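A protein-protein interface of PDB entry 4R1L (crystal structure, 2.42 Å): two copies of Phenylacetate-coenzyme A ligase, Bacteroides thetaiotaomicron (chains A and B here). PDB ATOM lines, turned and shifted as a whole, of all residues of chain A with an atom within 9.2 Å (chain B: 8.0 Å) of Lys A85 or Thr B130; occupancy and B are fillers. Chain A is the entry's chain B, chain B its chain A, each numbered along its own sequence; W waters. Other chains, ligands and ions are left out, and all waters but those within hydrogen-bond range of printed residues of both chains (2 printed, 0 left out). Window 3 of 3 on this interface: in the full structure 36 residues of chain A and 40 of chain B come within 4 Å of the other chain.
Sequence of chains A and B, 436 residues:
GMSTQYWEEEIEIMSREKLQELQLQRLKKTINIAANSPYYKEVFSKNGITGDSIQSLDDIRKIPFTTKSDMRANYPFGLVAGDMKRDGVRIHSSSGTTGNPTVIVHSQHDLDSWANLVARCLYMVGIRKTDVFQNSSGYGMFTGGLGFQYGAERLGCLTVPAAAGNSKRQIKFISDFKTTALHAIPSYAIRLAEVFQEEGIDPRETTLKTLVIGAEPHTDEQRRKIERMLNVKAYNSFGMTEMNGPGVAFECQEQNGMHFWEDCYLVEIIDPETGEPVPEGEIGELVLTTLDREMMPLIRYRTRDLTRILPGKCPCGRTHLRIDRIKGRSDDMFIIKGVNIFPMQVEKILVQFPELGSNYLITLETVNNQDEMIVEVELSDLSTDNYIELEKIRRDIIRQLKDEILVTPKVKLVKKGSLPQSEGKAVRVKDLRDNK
Among the printed residues, pairs that only touch across the chains: Arg A86 with Lys B129, Lys A85 with Thr B130, Gly A88 with Gly B156, Gly A88 with Cys B157, Met A84 with Leu B158, Val A105 with Leu B158, Val A89 with Leu B158 and Val A89 with Gly B156.
Of chain B, only Lys B129 and Thr B130 come within 4 Å of Lys A85.
Thr B130 touches one residue of chain A.
No residue of chain A comes within 4 Å of Asp B131.
Printed residues of chain A within 4 Å of Gly B156: Gly A88 and Val A89.
Of the printed residues of chain A, Lys B129 touches Lys A85 and Arg A86.
Of the printed residues of chain B, Val A89 touches Gly B156 (3.9 Å), Cys B157 (3.2 Å) and Leu B158 (3.9 Å).
Of the printed residues of chain B, Gly A88 touches Gly B156 (3.6 Å), Cys B157 (3.6 Å) and Leu B158 (3.2 Å).
Val A80 touches none of the printed residues of chain B.
The nearest printed residue of chain A that does not touch Thr B130 is Arg A86 (5.3 Å).
No position is printed for both chains.
Of the 11 pairs that touch across the chains among the printed residues, none has its exchanged pair printed and touching as well.
The side-chain sulfur (SG) of Cys B157 is in hydrogen-bond range of the backbone carbonyl oxygen (O) of Arg B128, 3.3 Å away.
O of Asp B131 sits at hydrogen-bond distance from N of Leu B158.
N of Phe B133 lies within hydrogen-bond range of O of Leu B158, at 2.9 Å.
The side-chain carboxylate (OD1) of Asp A83 lies within hydrogen-bond range of the backbone NH (N) of Arg A86 (3.4 Å).
N of Met A84 lies close to SD of Met A295 (3.7 Å).
The backbone NH (N) of Val A89 sits at hydrogen-bond distance from the backbone carbonyl oxygen (O) of His A106, at 2.8 Å.
Of the 14 printed residues of chain B, 5 touch a printed residue of chain A.
Hydrophobic or aromatic side chains of chain B that line the printed part of chain A: Leu B158.
Hydrophobic or aromatic side chains of chain A within 4 Å of the printed part of chain B: Met A84, Val A89 and Val A105.
Among the printed residues, no Asp or Glu carboxylate lies within 4 Å of a Lys or Arg side-chain nitrogen of the other chain.
The backbone carbonyl oxygen of Gly A88 sits close to the backbone NH of Leu B158 (3.4 Å).
The backbone carbonyl oxygen (O) of Lys A85 lies close to the backbone carbonyl oxygen (O) of Lys B129, at 3.2 Å.
The backbone carbonyl oxygen (O) of Val A89 lies close to the backbone carbonyl oxygen (O) of Cys B157 (3.3 Å).
Water W2 lies within hydrogen-bond range of OD1 of Asp A87 (2.6 Å), NZ of Lys B129 (3.1 Å) and NH1 of Arg A86 (3.3 Å).
Water W1 bridges the backbone carbonyl oxygen of Gly B156 (2.8 Å) and the backbone carbonyl oxygen of Arg A86 (3.0 Å).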
ATOM      1  N   PHE A  77      -7.778   3.753  -5.919  1.00  0.00           N
ATOM      2  CA  PHE A  77      -7.989   2.791  -6.981  1.00  0.00           C
ATOM      3  C   PHE A  77      -8.247   3.376  -8.383  1.00  0.00           C
ATOM      4  O   PHE A  77      -8.733   2.630  -9.242  1.00  0.00           O
ATOM      5  CB  PHE A  77      -9.200   1.907  -6.622  1.00  0.00           C
ATOM      6  CG  PHE A  77      -9.120   1.257  -5.260  1.00  0.00           C
ATOM      7  CD1 PHE A  77      -8.055   0.425  -4.927  1.00  0.00           C
ATOM      8  CD2 PHE A  77     -10.140   1.427  -4.334  1.00  0.00           C
ATOM      9  CE1 PHE A  77      -7.993  -0.181  -3.663  1.00  0.00           C
ATOM     10  CE2 PHE A  77     -10.091   0.800  -3.095  1.00  0.00           C
ATOM     11  CZ  PHE A  77      -9.014   0.009  -2.757  1.00  0.00           C
ATOM     12  N   VAL A  80      -6.775   1.024 -11.037  1.00  0.00           N
ATOM     13  CA  VAL A  80      -7.189  -0.388 -11.017  1.00  0.00           C
ATOM     14  C   VAL A  80      -7.929  -0.640 -12.333  1.00  0.00           C
ATOM     15  O   VAL A  80      -8.953   0.010 -12.606  1.00  0.00           O
ATOM     16  CB  VAL A  80      -8.019  -0.820  -9.753  1.00  0.00           C
ATOM     17  CG1 VAL A  80      -8.553  -2.249  -9.884  1.00  0.00           C
ATOM     18  CG2 VAL A  80      -7.198  -0.702  -8.484  1.00  0.00           C
ATOM     19  N   GLY A  82      -8.553  -4.133 -13.587  1.00  0.00           N
ATOM     20  CA  GLY A  82      -9.362  -5.344 -13.496  1.00  0.00           C
ATOM     21  C   GLY A  82     -10.595  -5.239 -12.619  1.00  0.00           C
ATOM     22  O   GLY A  82     -10.979  -4.152 -12.183  1.00  0.00           O
ATOM     23  N   ASP A  83     -11.247  -6.383 -12.384  1.00  0.00           N
ATOM     24  CA  ASP A  83     -12.434  -6.498 -11.545  1.00  0.00           C
ATOM     25  C   ASP A  83     -11.963  -6.861 -10.149  1.00  0.00           C
ATOM     26  O   ASP A  83     -11.736  -8.031  -9.828  1.00  0.00           O
ATOM     27  CB  ASP A  83     -13.414  -7.524 -12.129  1.00  0.00           C
ATOM     28  CG  ASP A  83     -14.753  -7.638 -11.431  1.00  0.00           C
ATOM     29  OD1 ASP A  83     -14.938  -6.997 -10.374  1.00  0.00           O
ATOM     30  OD2 ASP A  83     -15.623  -8.347 -11.950  1.00  0.00           O
ATOM     31  N   MET A  84     -11.758  -5.840  -9.346  1.00  0.00           N
ATOM     32  CA  MET A  84     -11.217  -5.926  -8.007  1.00  0.00           C
ATOM     33  C   MET A  84     -12.121  -6.741  -7.076  1.00  0.00           C
ATOM     34  O   MET A  84     -11.608  -7.585  -6.346  1.00  0.00           O
ATOM     35  CB  MET A  84     -11.035  -4.498  -7.474  1.00  0.00           C
ATOM     36  CG  MET A  84     -10.348  -4.428  -6.146  1.00  0.00           C
ATOM     37  SD  MET A  84      -9.899  -2.623  -5.649  1.00  0.00           S
ATOM     38  CE  MET A  84     -11.513  -1.783  -5.659  1.00  0.00           C
ATOM     39  N   LYS A  85     -13.449  -6.534  -7.138  1.00  0.00           N
ATOM     40  CA  LYS A  85     -14.413  -7.237  -6.284  1.00  0.00           C
ATOM     41  C   LYS A  85     -14.363  -8.766  -6.523  1.00  0.00           C
ATOM     42  O   LYS A  85     -14.360  -9.529  -5.559  1.00  0.00           O
ATOM     43  CB  LYS A  85     -15.823  -6.690  -6.562  1.00  0.00           C
ATOM     44  CG  LYS A  85     -16.895  -7.068  -5.557  1.00  0.00           C
ATOM     45  CD  LYS A  85     -18.220  -6.373  -5.880  1.00  0.00           C
ATOM     46  CE  LYS A  85     -19.288  -6.752  -4.890  1.00  0.00           C
ATOM     47  NZ  LYS A  85     -20.600  -6.153  -5.237  1.00  0.00           N
ATOM     48  N   ARG A  86     -14.281  -9.186  -7.794  1.00  0.00           N
ATOM     49  CA  ARG A  86     -14.269 -10.596  -8.185  1.00  0.00           C
ATOM     50  C   ARG A  86     -12.852 -11.193  -8.210  1.00  0.00           C
ATOM     51  O   ARG A  86     -12.662 -12.322  -7.763  1.00  0.00           O
ATOM     52  CB  ARG A  86     -14.898 -10.732  -9.589  1.00  0.00           C
ATOM     53  CG  ARG A  86     -15.126 -12.155 -10.082  1.00  0.00           C
ATOM     54  CD  ARG A  86     -15.443 -12.167 -11.569  1.00  0.00           C
ATOM     55  NE  ARG A  86     -15.860 -13.487 -12.043  1.00  0.00           N
ATOM     56  CZ  ARG A  86     -15.033 -14.441 -12.459  1.00  0.00           C
ATOM     57  NH1 ARG A  86     -13.720 -14.242 -12.450  1.00  0.00           N
ATOM     58  NH2 ARG A  86     -15.511 -15.607 -12.867  1.00  0.00           N
ATOM     59  N   ASP A  87     -11.872 -10.477  -8.756  1.00  0.00           N
ATOM     60  CA  ASP A  87     -10.549 -11.061  -8.930  1.00  0.00           C
ATOM     61  C   ASP A  87      -9.427 -10.471  -8.058  1.00  0.00           C
ATOM     62  O   ASP A  87      -8.361 -11.080  -8.030  1.00  0.00           O
ATOM     63  CB  ASP A  87     -10.143 -10.873 -10.411  1.00  0.00           C
ATOM     64  CG  ASP A  87     -11.128 -11.495 -11.409  1.00  0.00           C
ATOM     65  OD1 ASP A  87     -11.739 -12.557 -11.077  1.00  0.00           O
ATOM     66  OD2 ASP A  87     -11.258 -10.949 -12.540  1.00  0.00           O
ATOM     67  N   GLY A  88      -9.660  -9.361  -7.355  1.00  0.00           N
ATOM     68  CA  GLY A  88      -8.659  -8.734  -6.481  1.00  0.00           C
ATOM     69  C   GLY A  88      -8.475  -9.551  -5.222  1.00  0.00           C
ATOM     70  O   GLY A  88      -9.470  -9.833  -4.544  1.00  0.00           O
ATOM     71  N   VAL A  89      -7.219  -9.996  -4.926  1.00  0.00           N
ATOM     72  CA  VAL A  89      -6.987 -10.855  -3.756  1.00  0.00           C
ATOM     73  C   VAL A  89      -5.990 -10.197  -2.725  1.00  0.00           C
ATOM     74  O   VAL A  89      -5.842 -10.721  -1.620  1.00  0.00           O
ATOM     75  CB  VAL A  89      -6.496 -12.280  -4.146  1.00  0.00           C
ATOM     76  CG1 VAL A  89      -7.507 -12.986  -5.030  1.00  0.00           C
ATOM     77  CG2 VAL A  89      -5.137 -12.247  -4.822  1.00  0.00           C
ATOM     78  N   VAL A 105      -2.884  -3.142  -6.117  1.00  0.00           N
ATOM     79  CA  VAL A 105      -3.878  -4.196  -6.005  1.00  0.00           C
ATOM     80  C   VAL A 105      -3.480  -5.322  -6.947  1.00  0.00           C
ATOM     81  O   VAL A 105      -3.164  -5.084  -8.119  1.00  0.00           O
ATOM     82  CB  VAL A 105      -5.302  -3.674  -6.277  1.00  0.00           C
ATOM     83  CG1 VAL A 105      -6.336  -4.756  -5.953  1.00  0.00           C
ATOM     84  CG2 VAL A 105      -5.567  -2.432  -5.441  1.00  0.00           C
ATOM     85  N   HIS A 106      -3.447  -6.546  -6.398  1.00  0.00           N
ATOM     86  CA  HIS A 106      -3.088  -7.776  -7.100  1.00  0.00           C
ATOM     87  C   HIS A 106      -4.237  -8.753  -7.195  1.00  0.00           C
ATOM     88  O   HIS A 106      -5.022  -8.891  -6.260  1.00  0.00           O
ATOM     89  CB  HIS A 106      -1.927  -8.497  -6.370  1.00  0.00           C
ATOM     90  CG  HIS A 106      -0.646  -7.723  -6.299  1.00  0.00           C
ATOM     91  ND1 HIS A 106       0.340  -7.861  -7.275  1.00  0.00           N
ATOM     92  CD2 HIS A 106      -0.222  -6.834  -5.365  1.00  0.00           C
ATOM     93  CE1 HIS A 106       1.318  -7.044  -6.911  1.00  0.00           C
ATOM     94  NE2 HIS A 106       1.023  -6.392  -5.775  1.00  0.00           N
ATOM     95  N   MET A 295      -4.327  -6.826 -12.668  1.00  0.00           N
ATOM     96  CA  MET A 295      -5.292  -6.066 -11.863  1.00  0.00           C
ATOM     97  C   MET A 295      -4.996  -4.572 -11.923  1.00  0.00           C
ATOM     98  O   MET A 295      -5.905  -3.760 -12.135  1.00  0.00           O
ATOM     99  CB  MET A 295      -5.270  -6.566 -10.400  1.00  0.00           C
ATOM    100  CG  MET A 295      -6.235  -5.838  -9.459  1.00  0.00           C
ATOM    101  SD  MET A 295      -8.085  -5.803 -10.024  1.00  0.00           S
ATOM    102  CE  MET A 295      -8.347  -7.683 -10.168  1.00  0.00           C
ATOM    103  N   GLY B 126     -20.521 -16.581   6.106  1.00  0.00           N
ATOM    104  CA  GLY B 126     -21.031 -15.739   5.034  1.00  0.00           C
ATOM    105  C   GLY B 126     -20.066 -14.879   4.245  1.00  0.00           C
ATOM    106  O   GLY B 126     -20.517 -14.061   3.424  1.00  0.00           O
ATOM    107  N   ILE B 127     -18.746 -15.036   4.476  1.00  0.00           N
ATOM    108  CA  ILE B 127     -17.745 -14.265   3.769  1.00  0.00           C
ATOM    109  C   ILE B 127     -17.602 -14.895   2.370  1.00  0.00           C
ATOM    110  O   ILE B 127     -17.644 -16.124   2.241  1.00  0.00           O
ATOM    111  CB  ILE B 127     -16.409 -14.177   4.565  1.00  0.00           C
ATOM    112  CG1 ILE B 127     -16.643 -13.527   5.948  1.00  0.00           C
ATOM    113  CG2 ILE B 127     -15.354 -13.393   3.793  1.00  0.00           C
ATOM    114  CD1 ILE B 127     -15.456 -13.579   6.956  1.00  0.00           C
ATOM    115  N   ARG B 128     -17.500 -14.026   1.320  1.00  0.00           N
ATOM    116  CA  ARG B 128     -17.357 -14.457  -0.073  1.00  0.00           C
ATOM    117  C   ARG B 128     -16.133 -13.796  -0.706  1.00  0.00           C
ATOM    118  O   ARG B 128     -15.489 -12.953  -0.078  1.00  0.00           O
ATOM    119  CB  ARG B 128     -18.633 -14.139  -0.876  1.00  0.00           C
ATOM    120  CG  ARG B 128     -19.906 -14.871  -0.376  1.00  0.00           C
ATOM    121  CD  ARG B 128     -19.856 -16.386  -0.498  1.00  0.00           C
ATOM    122  NE  ARG B 128     -21.070 -17.023   0.027  1.00  0.00           N
ATOM    123  CZ  ARG B 128     -21.202 -17.541   1.248  1.00  0.00           C
ATOM    124  NH1 ARG B 128     -20.177 -17.542   2.094  1.00  0.00           N
ATOM    125  NH2 ARG B 128     -22.351 -18.086   1.621  1.00  0.00           N
ATOM    126  N   LYS B 129     -15.797 -14.184  -1.945  1.00  0.00           N
ATOM    127  CA  LYS B 129     -14.651 -13.608  -2.665  1.00  0.00           C
ATOM    128  C   LYS B 129     -14.871 -12.088  -2.886  1.00  0.00           C
ATOM    129  O   LYS B 129     -13.894 -11.350  -2.963  1.00  0.00           O
ATOM    130  CB  LYS B 129     -14.415 -14.341  -4.010  1.00  0.00           C
ATOM    131  CG  LYS B 129     -15.564 -14.241  -5.016  1.00  0.00           C
ATOM    132  CD  LYS B 129     -15.415 -15.184  -6.210  1.00  0.00           C
ATOM    133  CE  LYS B 129     -14.290 -14.859  -7.162  1.00  0.00           C
ATOM    134  NZ  LYS B 129     -14.270 -15.706  -8.380  1.00  0.00           N
ATOM    135  N   THR B 130     -16.146 -11.630  -2.911  1.00  0.00           N
ATOM    136  CA  THR B 130     -16.539 -10.238  -3.122  1.00  0.00           C
ATOM    137  C   THR B 130     -16.223  -9.363  -1.905  1.00  0.00           C
ATOM    138  O   THR B 130     -16.297  -8.127  -1.996  1.00  0.00           O
ATOM    139  CB  THR B 130     -18.042 -10.139  -3.455  1.00  0.00           C
ATOM    140  OG1 THR B 130     -18.851 -10.725  -2.406  1.00  0.00           O
ATOM    141  CG2 THR B 130     -18.369 -10.742  -4.815  1.00  0.00           C
ATOM    142  N   ASP B 131     -15.869  -9.990  -0.778  1.00  0.00           N
ATOM    143  CA  ASP B 131     -15.574  -9.269   0.449  1.00  0.00           C
ATOM    144  C   ASP B 131     -14.129  -8.737   0.463  1.00  0.00           C
ATOM    145  O   ASP B 131     -13.228  -9.287  -0.188  1.00  0.00           O
ATOM    146  CB  ASP B 131     -15.819 -10.186   1.666  1.00  0.00           C
ATOM    147  CG  ASP B 131     -17.284 -10.329   2.036  1.00  0.00           C
ATOM    148  OD1 ASP B 131     -17.823  -9.404   2.657  1.00  0.00           O
ATOM    149  OD2 ASP B 131     -17.874 -11.405   1.761  1.00  0.00           O
ATOM    150  N   VAL B 132     -13.928  -7.662   1.240  1.00  0.00           N
ATOM    151  CA  VAL B 132     -12.626  -7.047   1.500  1.00  0.00           C
ATOM    152  C   VAL B 132     -12.260  -7.459   2.933  1.00  0.00           C
ATOM    153  O   VAL B 132     -12.889  -6.993   3.883  1.00  0.00           O
ATOM    154  CB  VAL B 132     -12.607  -5.516   1.258  1.00  0.00           C
ATOM    155  CG1 VAL B 132     -11.205  -4.944   1.471  1.00  0.00           C
ATOM    156  CG2 VAL B 132     -13.128  -5.171  -0.142  1.00  0.00           C
ATOM    157  N   PHE B 133     -11.312  -8.399   3.067  1.00  0.00           N
ATOM    158  CA  PHE B 133     -10.924  -8.994   4.346  1.00  0.00           C
ATOM    159  C   PHE B 133      -9.661  -8.345   4.921  1.00  0.00           C
ATOM    160  O   PHE B 133      -8.592  -8.485   4.341  1.00  0.00           O
ATOM    161  CB  PHE B 133     -10.696 -10.514   4.172  1.00  0.00           C
ATOM    162  CG  PHE B 133     -10.343 -11.222   5.456  1.00  0.00           C
ATOM    163  CD1 PHE B 133     -11.336 -11.674   6.312  1.00  0.00           C
ATOM    164  CD2 PHE B 133      -9.016 -11.443   5.808  1.00  0.00           C
ATOM    165  CE1 PHE B 133     -11.010 -12.327   7.497  1.00  0.00           C
ATOM    166  CE2 PHE B 133      -8.685 -12.091   7.004  1.00  0.00           C
ATOM    167  CZ  PHE B 133      -9.684 -12.539   7.832  1.00  0.00           C
ATOM    168  N   LEU B 155     -10.170 -18.347  -0.407  1.00  0.00           N
ATOM    169  CA  LEU B 155     -11.582 -18.025  -0.599  1.00  0.00           C
ATOM    170  C   LEU B 155     -11.729 -16.974  -1.772  1.00  0.00           C
ATOM    171  O   LEU B 155     -12.697 -17.029  -2.540  1.00  0.00           O
ATOM    172  CB  LEU B 155     -12.170 -17.522   0.735  1.00  0.00           C
ATOM    173  CG  LEU B 155     -13.584 -16.951   0.790  1.00  0.00           C
ATOM    174  CD1 LEU B 155     -14.621 -17.869   0.118  1.00  0.00           C
ATOM    175  CD2 LEU B 155     -13.983 -16.700   2.223  1.00  0.00           C
ATOM    176  N   GLY B 156     -10.753 -16.086  -1.925  1.00  0.00           N
ATOM    177  CA  GLY B 156     -10.747 -15.127  -3.022  1.00  0.00           C
ATOM    178  C   GLY B 156     -11.009 -13.688  -2.632  1.00  0.00           C
ATOM    179  O   GLY B 156     -11.141 -12.829  -3.515  1.00  0.00           O
ATOM    180  N   CYS B 157     -11.078 -13.419  -1.301  1.00  0.00           N
ATOM    181  CA  CYS B 157     -11.289 -12.082  -0.745  1.00  0.00           C
ATOM    182  C   CYS B 157     -10.197 -11.136  -1.198  1.00  0.00           C
ATOM    183  O   CYS B 157      -9.052 -11.572  -1.379  1.00  0.00           O
ATOM    184  CB  CYS B 157     -11.322 -12.132   0.780  1.00  0.00           C
ATOM    185  SG  CYS B 157     -12.579 -13.219   1.474  1.00  0.00           S
ATOM    186  N   LEU B 158     -10.524  -9.833  -1.286  1.00  0.00           N
ATOM    187  CA  LEU B 158      -9.516  -8.792  -1.473  1.00  0.00           C
ATOM    188  C   LEU B 158      -8.904  -8.608  -0.085  1.00  0.00           C
ATOM    189  O   LEU B 158      -9.589  -8.109   0.807  1.00  0.00           O
ATOM    190  CB  LEU B 158     -10.094  -7.511  -2.089  1.00  0.00           C
ATOM    191  CG  LEU B 158      -9.128  -6.336  -2.188  1.00  0.00           C
ATOM    192  CD1 LEU B 158      -7.997  -6.614  -3.159  1.00  0.00           C
ATOM    193  CD2 LEU B 158      -9.847  -5.088  -2.575  1.00  0.00           C
ATOM    194  N   LYS B 178     -12.725  -0.013   1.751  1.00  0.00           N
ATOM    195  CA  LYS B 178     -14.118  -0.434   1.971  1.00  0.00           C
ATOM    196  C   LYS B 178     -14.151  -1.880   2.491  1.00  0.00           C
ATOM    197  O   LYS B 178     -14.829  -2.745   1.919  1.00  0.00           O
ATOM    198  CB  LYS B 178     -15.006  -0.275   0.697  1.00  0.00           C
ATOM    199  CG  LYS B 178     -14.907   1.055  -0.042  1.00  0.00           C
ATOM    200  CD  LYS B 178     -15.205   2.265   0.825  1.00  0.00           C
ATOM    201  CE  LYS B 178     -14.995   3.552   0.080  1.00  0.00           C
ATOM    202  NZ  LYS B 178     -15.067   4.710   1.005  1.00  0.00           N
ATOM    203  N   THR B 180     -15.012  -5.139   4.583  1.00  0.00           N
ATOM    204  CA  THR B 180     -16.321  -5.692   4.959  1.00  0.00           C
ATOM    205  C   THR B 180     -16.161  -6.802   6.006  1.00  0.00           C
ATOM    206  O   THR B 180     -17.090  -7.042   6.786  1.00  0.00           O
ATOM    207  CB  THR B 180     -17.066  -6.210   3.716  1.00  0.00           C
ATOM    208  OG1 THR B 180     -16.289  -7.211   3.083  1.00  0.00           O
ATOM    209  CG2 THR B 180     -17.361  -5.102   2.695  1.00  0.00           C
HETATM  210  O   HOH W   1     -10.573 -13.778  -6.116  1.00  0.00           O
HETATM  211  O   HOH W   2     -11.717 -14.853  -9.858  1.00  0.00           O
